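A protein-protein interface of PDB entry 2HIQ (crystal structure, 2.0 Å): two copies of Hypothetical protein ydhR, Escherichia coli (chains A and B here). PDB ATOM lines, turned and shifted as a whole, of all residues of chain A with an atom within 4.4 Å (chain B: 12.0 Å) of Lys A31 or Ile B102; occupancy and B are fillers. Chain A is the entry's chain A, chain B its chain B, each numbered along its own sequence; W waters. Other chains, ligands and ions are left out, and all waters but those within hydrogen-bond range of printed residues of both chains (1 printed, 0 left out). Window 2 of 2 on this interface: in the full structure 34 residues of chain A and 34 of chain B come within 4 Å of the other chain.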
ATOM      1  N   ALA A  27     -15.805  24.278   4.855  1.00  0.00           N
ATOM      2  CA  ALA A  27     -15.341  24.936   3.642  1.00  0.00           C
ATOM      3  C   ALA A  27     -14.648  23.943   2.712  1.00  0.00           C
ATOM      4  O   ALA A  27     -14.785  24.016   1.491  1.00  0.00           O
ATOM      5  CB  ALA A  27     -14.390  26.066   3.987  1.00  0.00           C
ATOM      6  N   GLU A  28     -13.901  23.017   3.296  1.00  0.00           N
ATOM      7  CA  GLU A  28     -13.194  22.018   2.510  1.00  0.00           C
ATOM      8  C   GLU A  28     -14.163  20.996   1.928  1.00  0.00           C
ATOM      9  O   GLU A  28     -14.066  20.625   0.762  1.00  0.00           O
ATOM     10  CB  GLU A  28     -12.169  21.295   3.383  1.00  0.00           C
ATOM     11  CG  GLU A  28     -11.440  20.171   2.670  1.00  0.00           C
ATOM     12  CD  GLU A  28     -10.943  19.110   3.630  1.00  0.00           C
ATOM     13  OE1 GLU A  28     -10.102  19.434   4.496  1.00  0.00           O
ATOM     14  OE2 GLU A  28     -11.399  17.952   3.522  1.00  0.00           O
ATOM     15  N   GLN A  29     -15.109  20.554   2.744  1.00  0.00           N
ATOM     16  CA  GLN A  29     -16.069  19.553   2.310  1.00  0.00           C
ATOM     17  C   GLN A  29     -17.096  20.071   1.308  1.00  0.00           C
ATOM     18  O   GLN A  29     -17.417  19.392   0.334  1.00  0.00           O
ATOM     19  CB  GLN A  29     -16.800  18.986   3.525  1.00  0.00           C
ATOM     20  CG  GLN A  29     -17.517  17.670   3.269  1.00  0.00           C
ATOM     21  CD  GLN A  29     -16.543  16.547   2.922  1.00  0.00           C
ATOM     22  OE1 GLN A  29     -15.441  16.475   3.472  1.00  0.00           O
ATOM     23  NE2 GLN A  29     -16.953  15.658   2.023  1.00  0.00           N
ATOM     24  N   LEU A  30     -17.607  21.274   1.538  1.00  0.00           N
ATOM     25  CA  LEU A  30     -18.624  21.819   0.651  1.00  0.00           C
ATOM     26  C   LEU A  30     -18.128  22.740  -0.459  1.00  0.00           C
ATOM     27  O   LEU A  30     -18.924  23.390  -1.139  1.00  0.00           O
ATOM     28  CB  LEU A  30     -19.704  22.515   1.485  1.00  0.00           C
ATOM     29  CG  LEU A  30     -20.439  21.574   2.453  1.00  0.00           C
ATOM     30  CD1 LEU A  30     -21.536  22.338   3.193  1.00  0.00           C
ATOM     31  CD2 LEU A  30     -21.044  20.407   1.682  1.00  0.00           C
ATOM     32  N   LYS A  31     -16.818  22.788  -0.658  1.00  0.00           N
ATOM     33  CA  LYS A  31     -16.255  23.632  -1.705  1.00  0.00           C
ATOM     34  C   LYS A  31     -16.874  23.341  -3.086  1.00  0.00           C
ATOM     35  O   LYS A  31     -17.246  24.268  -3.811  1.00  0.00           O
ATOM     36  CB  LYS A  31     -14.732  23.446  -1.742  1.00  0.00           C
ATOM     37  CG  LYS A  31     -13.994  24.250  -2.799  1.00  0.00           C
ATOM     38  CD  LYS A  31     -12.502  23.998  -2.665  1.00  0.00           C
ATOM     39  CE  LYS A  31     -11.704  24.652  -3.779  1.00  0.00           C
ATOM     40  NZ  LYS A  31     -11.806  26.139  -3.742  1.00  0.00           N
ATOM     41  N   PRO A  32     -16.992  22.050  -3.467  1.00  0.00           N
ATOM     42  CA  PRO A  32     -17.575  21.703  -4.773  1.00  0.00           C
ATOM     43  C   PRO A  32     -19.016  22.193  -4.885  1.00  0.00           C
ATOM     44  O   PRO A  32     -19.461  22.639  -5.945  1.00  0.00           O
ATOM     45  CB  PRO A  32     -17.497  20.178  -4.796  1.00  0.00           C
ATOM     46  CG  PRO A  32     -16.318  19.880  -3.921  1.00  0.00           C
ATOM     47  CD  PRO A  32     -16.515  20.839  -2.773  1.00  0.00           C
ATOM     48  N   LEU A  33     -19.746  22.091  -3.782  1.00  0.00           N
ATOM     49  CA  LEU A  33     -21.127  22.540  -3.766  1.00  0.00           C
ATOM     50  C   LEU A  33     -21.173  24.047  -4.006  1.00  0.00           C
ATOM     51  O   LEU A  33     -21.985  24.535  -4.790  1.00  0.00           O
ATOM     52  CB  LEU A  33     -21.763  22.199  -2.421  1.00  0.00           C
ATOM     53  CG  LEU A  33     -23.225  22.585  -2.242  1.00  0.00           C
ATOM     54  CD1 LEU A  33     -24.093  21.897  -3.289  1.00  0.00           C
ATOM     55  CD2 LEU A  33     -23.655  22.198  -0.842  1.00  0.00           C
ATOM     56  N   ALA A  34     -20.293  24.782  -3.331  1.00  0.00           N
ATOM     57  CA  ALA A  34     -20.247  26.233  -3.474  1.00  0.00           C
ATOM     58  C   ALA A  34     -19.945  26.642  -4.909  1.00  0.00           C
ATOM     59  O   ALA A  34     -20.572  27.556  -5.454  1.00  0.00           O
ATOM     60  CB  ALA A  34     -19.198  26.824  -2.531  1.00  0.00           C
ATOM     61  N   GLU A  35     -18.984  25.970  -5.533  1.00  0.00           N
ATOM     62  CA  GLU A  35     -18.635  26.301  -6.907  1.00  0.00           C
ATOM     63  C   GLU A  35     -19.802  26.059  -7.869  1.00  0.00           C
ATOM     64  O   GLU A  35     -19.972  26.806  -8.837  1.00  0.00           O
ATOM     65  CB  GLU A  35     -17.399  25.499  -7.340  1.00  0.00           C
ATOM     66  CG  GLU A  35     -16.172  25.772  -6.468  1.00  0.00           C
ATOM     67  CD  GLU A  35     -14.969  24.924  -6.845  1.00  0.00           C
ATOM     68  OE1 GLU A  35     -15.126  23.689  -6.973  1.00  0.00           O
ATOM     69  OE2 GLU A  35     -13.863  25.490  -6.994  1.00  0.00           O
ATOM     70  N   ASN A  38     -22.388  28.896  -8.297  1.00  0.00           N
ATOM     71  CA  ASN A  38     -22.016  29.989  -9.194  1.00  0.00           C
ATOM     72  C   ASN A  38     -22.522  29.801 -10.630  1.00  0.00           C
ATOM     73  O   ASN A  38     -22.605  30.770 -11.388  1.00  0.00           O
ATOM     74  CB  ASN A  38     -20.500  30.199  -9.200  1.00  0.00           C
ATOM     75  CG  ASN A  38     -19.993  30.823  -7.905  1.00  0.00           C
ATOM     76  OD1 ASN A  38     -20.689  31.626  -7.273  1.00  0.00           O
ATOM     77  ND2 ASN A  38     -18.777  30.470  -7.513  1.00  0.00           N
ATOM     78  N   VAL B  95     -20.671  33.186  10.089  1.00  0.00           N
ATOM     79  CA  VAL B  95     -20.555  33.155   8.640  1.00  0.00           C
ATOM     80  C   VAL B  95     -19.323  32.341   8.243  1.00  0.00           C
ATOM     81  O   VAL B  95     -18.255  32.495   8.841  1.00  0.00           O
ATOM     82  CB  VAL B  95     -20.404  34.582   8.071  1.00  0.00           C
ATOM     83  CG1 VAL B  95     -20.060  34.527   6.595  1.00  0.00           C
ATOM     84  CG2 VAL B  95     -21.692  35.370   8.288  1.00  0.00           C
ATOM     85  N   ASN B  96     -19.463  31.465   7.250  1.00  0.00           N
ATOM     86  CA  ASN B  96     -18.309  30.694   6.793  1.00  0.00           C
ATOM     87  C   ASN B  96     -17.672  31.562   5.711  1.00  0.00           C
ATOM     88  O   ASN B  96     -18.190  31.651   4.602  1.00  0.00           O
ATOM     89  CB  ASN B  96     -18.732  29.348   6.199  1.00  0.00           C
ATOM     90  CG  ASN B  96     -17.541  28.437   5.922  1.00  0.00           C
ATOM     91  OD1 ASN B  96     -17.245  27.528   6.700  1.00  0.00           O
ATOM     92  ND2 ASN B  96     -16.844  28.692   4.820  1.00  0.00           N
ATOM     93  N   GLU B  97     -16.552  32.198   6.036  1.00  0.00           N
ATOM     94  CA  GLU B  97     -15.877  33.090   5.101  1.00  0.00           C
ATOM     95  C   GLU B  97     -15.386  32.444   3.807  1.00  0.00           C
ATOM     96  O   GLU B  97     -15.618  32.971   2.723  1.00  0.00           O
ATOM     97  CB  GLU B  97     -14.684  33.775   5.781  1.00  0.00           C
ATOM     98  CG  GLU B  97     -14.979  34.437   7.126  1.00  0.00           C
ATOM     99  CD  GLU B  97     -16.062  35.499   7.055  1.00  0.00           C
ATOM    100  OE1 GLU B  97     -16.188  36.170   6.005  1.00  0.00           O
ATOM    101  OE2 GLU B  97     -16.782  35.678   8.065  1.00  0.00           O
ATOM    102  N   PRO B  98     -14.688  31.302   3.904  1.00  0.00           N
ATOM    103  CA  PRO B  98     -14.182  30.633   2.698  1.00  0.00           C
ATOM    104  C   PRO B  98     -15.266  30.390   1.634  1.00  0.00           C
ATOM    105  O   PRO B  98     -15.128  30.826   0.486  1.00  0.00           O
ATOM    106  CB  PRO B  98     -13.597  29.331   3.246  1.00  0.00           C
ATOM    107  CG  PRO B  98     -13.164  29.714   4.639  1.00  0.00           C
ATOM    108  CD  PRO B  98     -14.333  30.544   5.116  1.00  0.00           C
ATOM    109  N   LEU B  99     -16.341  29.704   2.020  1.00  0.00           N
ATOM    110  CA  LEU B  99     -17.435  29.403   1.093  1.00  0.00           C
ATOM    111  C   LEU B  99     -18.134  30.683   0.609  1.00  0.00           C
ATOM    112  O   LEU B  99     -18.494  30.792  -0.563  1.00  0.00           O
ATOM    113  CB  LEU B  99     -18.438  28.438   1.760  1.00  0.00           C
ATOM    114  CG  LEU B  99     -17.884  27.055   2.162  1.00  0.00           C
ATOM    115  CD1 LEU B  99     -18.912  26.265   2.983  1.00  0.00           C
ATOM    116  CD2 LEU B  99     -17.512  26.273   0.905  1.00  0.00           C
ATOM    117  N   SER B 100     -18.313  31.657   1.503  1.00  0.00           N
ATOM    118  CA  SER B 100     -18.958  32.912   1.126  1.00  0.00           C
ATOM    119  C   SER B 100     -18.128  33.651   0.071  1.00  0.00           C
ATOM    120  O   SER B 100     -18.679  34.252  -0.855  1.00  0.00           O
ATOM    121  CB  SER B 100     -19.170  33.790   2.361  1.00  0.00           C
ATOM    122  OG  SER B 100     -20.126  33.194   3.238  1.00  0.00           O
ATOM    123  N   GLN B 101     -16.803  33.603   0.203  1.00  0.00           N
ATOM    124  CA  GLN B 101     -15.926  34.257  -0.771  1.00  0.00           C
ATOM    125  C   GLN B 101     -16.064  33.589  -2.139  1.00  0.00           C
ATOM    126  O   GLN B 101     -16.024  34.255  -3.175  1.00  0.00           O
ATOM    127  CB  GLN B 101     -14.464  34.194  -0.317  1.00  0.00           C
ATOM    128  CG  GLN B 101     -14.103  35.163   0.798  1.00  0.00           C
ATOM    129  CD  GLN B 101     -12.645  35.042   1.227  1.00  0.00           C
ATOM    130  OE1 GLN B 101     -12.270  34.128   1.974  1.00  0.00           O
ATOM    131  NE2 GLN B 101     -11.813  35.960   0.740  1.00  0.00           N
ATOM    132  N   ILE B 102     -16.223  32.271  -2.145  1.00  0.00           N
ATOM    133  CA  ILE B 102     -16.378  31.559  -3.406  1.00  0.00           C
ATOM    134  C   ILE B 102     -17.629  32.054  -4.125  1.00  0.00           C
ATOM    135  O   ILE B 102     -17.627  32.247  -5.342  1.00  0.00           O
ATOM    136  CB  ILE B 102     -16.468  30.025  -3.174  1.00  0.00           C
ATOM    137  CG1 ILE B 102     -15.099  29.503  -2.732  1.00  0.00           C
ATOM    138  CG2 ILE B 102     -16.900  29.309  -4.456  1.00  0.00           C
ATOM    139  CD1 ILE B 102     -15.095  28.055  -2.314  1.00  0.00           C
ATOM    140  N   ASN B 103     -18.685  32.300  -3.355  1.00  0.00           N
ATOM    141  CA  ASN B 103     -19.955  32.752  -3.914  1.00  0.00           C
ATOM    142  C   ASN B 103     -20.231  34.263  -3.927  1.00  0.00           C
ATOM    143  O   ASN B 103     -21.345  34.700  -3.632  1.00  0.00           O
ATOM    144  CB  ASN B 103     -21.094  32.015  -3.211  1.00  0.00           C
ATOM    145  CG  ASN B 103     -21.086  30.531  -3.522  1.00  0.00           C
ATOM    146  OD1 ASN B 103     -20.999  30.141  -4.692  1.00  0.00           O
ATOM    147  ND2 ASN B 103     -21.181  29.697  -2.493  1.00  0.00           N
ATOM    148  N   GLN B 104     -19.220  35.049  -4.287  1.00  0.00           N
ATOM    149  CA  GLN B 104     -19.359  36.499  -4.385  1.00  0.00           C
ATOM    150  C   GLN B 104     -18.410  37.028  -5.451  1.00  0.00           C
ATOM    151  O   GLN B 104     -17.646  36.207  -6.010  1.00  0.00           O
ATOM    152  CB  GLN B 104     -19.048  37.176  -3.054  1.00  0.00           C
ATOM    153  CG  GLN B 104     -20.021  36.851  -1.946  1.00  0.00           C
ATOM    154  CD  GLN B 104     -19.826  37.743  -0.737  1.00  0.00           C
ATOM    155  OE1 GLN B 104     -18.723  37.840  -0.193  1.00  0.00           O
ATOM    156  NE2 GLN B 104     -20.899  38.402  -0.308  1.00  0.00           N
HETATM  157  O   HOH W   1     -19.665  34.270  -7.149  1.00  0.00           O
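O of Ala A34 sits close to OD1 of Asn B103 (2.7 Å).
OD1 of Asn A38 lies close to OD1 of Asn B103.
The backbone carbonyl oxygen (O) of Ile B102 sits at hydrogen-bond distance from the side-chain amide nitrogen (ND2) of Asn A38 (3.0 Å).
No position is printed for both chains.
Of the printed residues of chain B, Lys A31 touches Leu B99 and Ile B102.
Of the printed residues of chain A, Ile B102 touches Lys A31 (3.99 Å), Ala A34 (3.9 Å) and Asn A38 (3.0 Å).
Of the printed residues of chain B, Ala A27 touches Asn B96 (3.7 Å), Pro B98 (3.4 Å) and Leu B99 (3.6 Å).
No residue of chain B comes within 4 Å of Gln A29.
Pro A32 touches none of the printed residues of chain B.
Of chain B, only Leu B99, Ile B102 and Asn B103 come within 4 Å of Ala A34.
No residue of chain B comes within 4 Å of Glu A35.
Of the printed residues of chain A, Asn B103 touches Ala A34 and Asn A38.
Of the printed residues of chain A, Asn B96 touches Ala A27 (3.7 Å).
Of the printed residues of chain A, Pro B98 touches Ala A27 (3.4 Å).
Printed residues of chain A within 4 Å of Leu B99: Ala A27, Leu A30, Lys A31 and Ala A34.
The nearest printed residue of chain B that does not touch Asn A38 is Gln B104 (4.8 Å).
Hydrophobic or aromatic side chains of chain B that line the printed part of chain A: Pro B98, Leu B99 and Ile B102.
Among the printed residues, 11 pairs touch across the chains.
Among the printed residues, no Asp or Glu carboxylate lies within 4 Å of a Lys or Arg side-chain nitrogen of the other chain.
Among the printed residues, pairs that only touch across the chains: Ala A27 with Asn B96 (3.7 Å), Ala A27 with Pro B98 (3.4 Å), Ala A27 with Leu B99 (3.6 Å), Leu A30 with Leu B99 (3.8 Å), Lys A31 with Leu B99 (3.9 Å), Lys A31 with Ile B102 (3.99 Å), Ala A34 with Leu B99 (3.9 Å) and Ala A34 with Ile B102 (3.9 Å).
ND2 of Asn B96 lies close to N of Leu B99.
The side-chain amino group of Lys A31 lies within salt-bridge range of the side-chain carboxylate of Glu A35 (3.9 Å).
The backbone carbonyl oxygen (O) of Leu B99 sits at hydrogen-bond distance from the side-chain amide nitrogen (ND2) of Asn B103, 3.5 Å away.
OG of Ser B100 lies within hydrogen-bond range of O of Asn B96 (2.8 Å).
Water W1 lies within hydrogen-bond range of the side-chain amide oxygen (OD1) of Asn A38, the backbone NH (N) of Gln B104 and the backbone carbonyl oxygen (O) of Ile B102.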
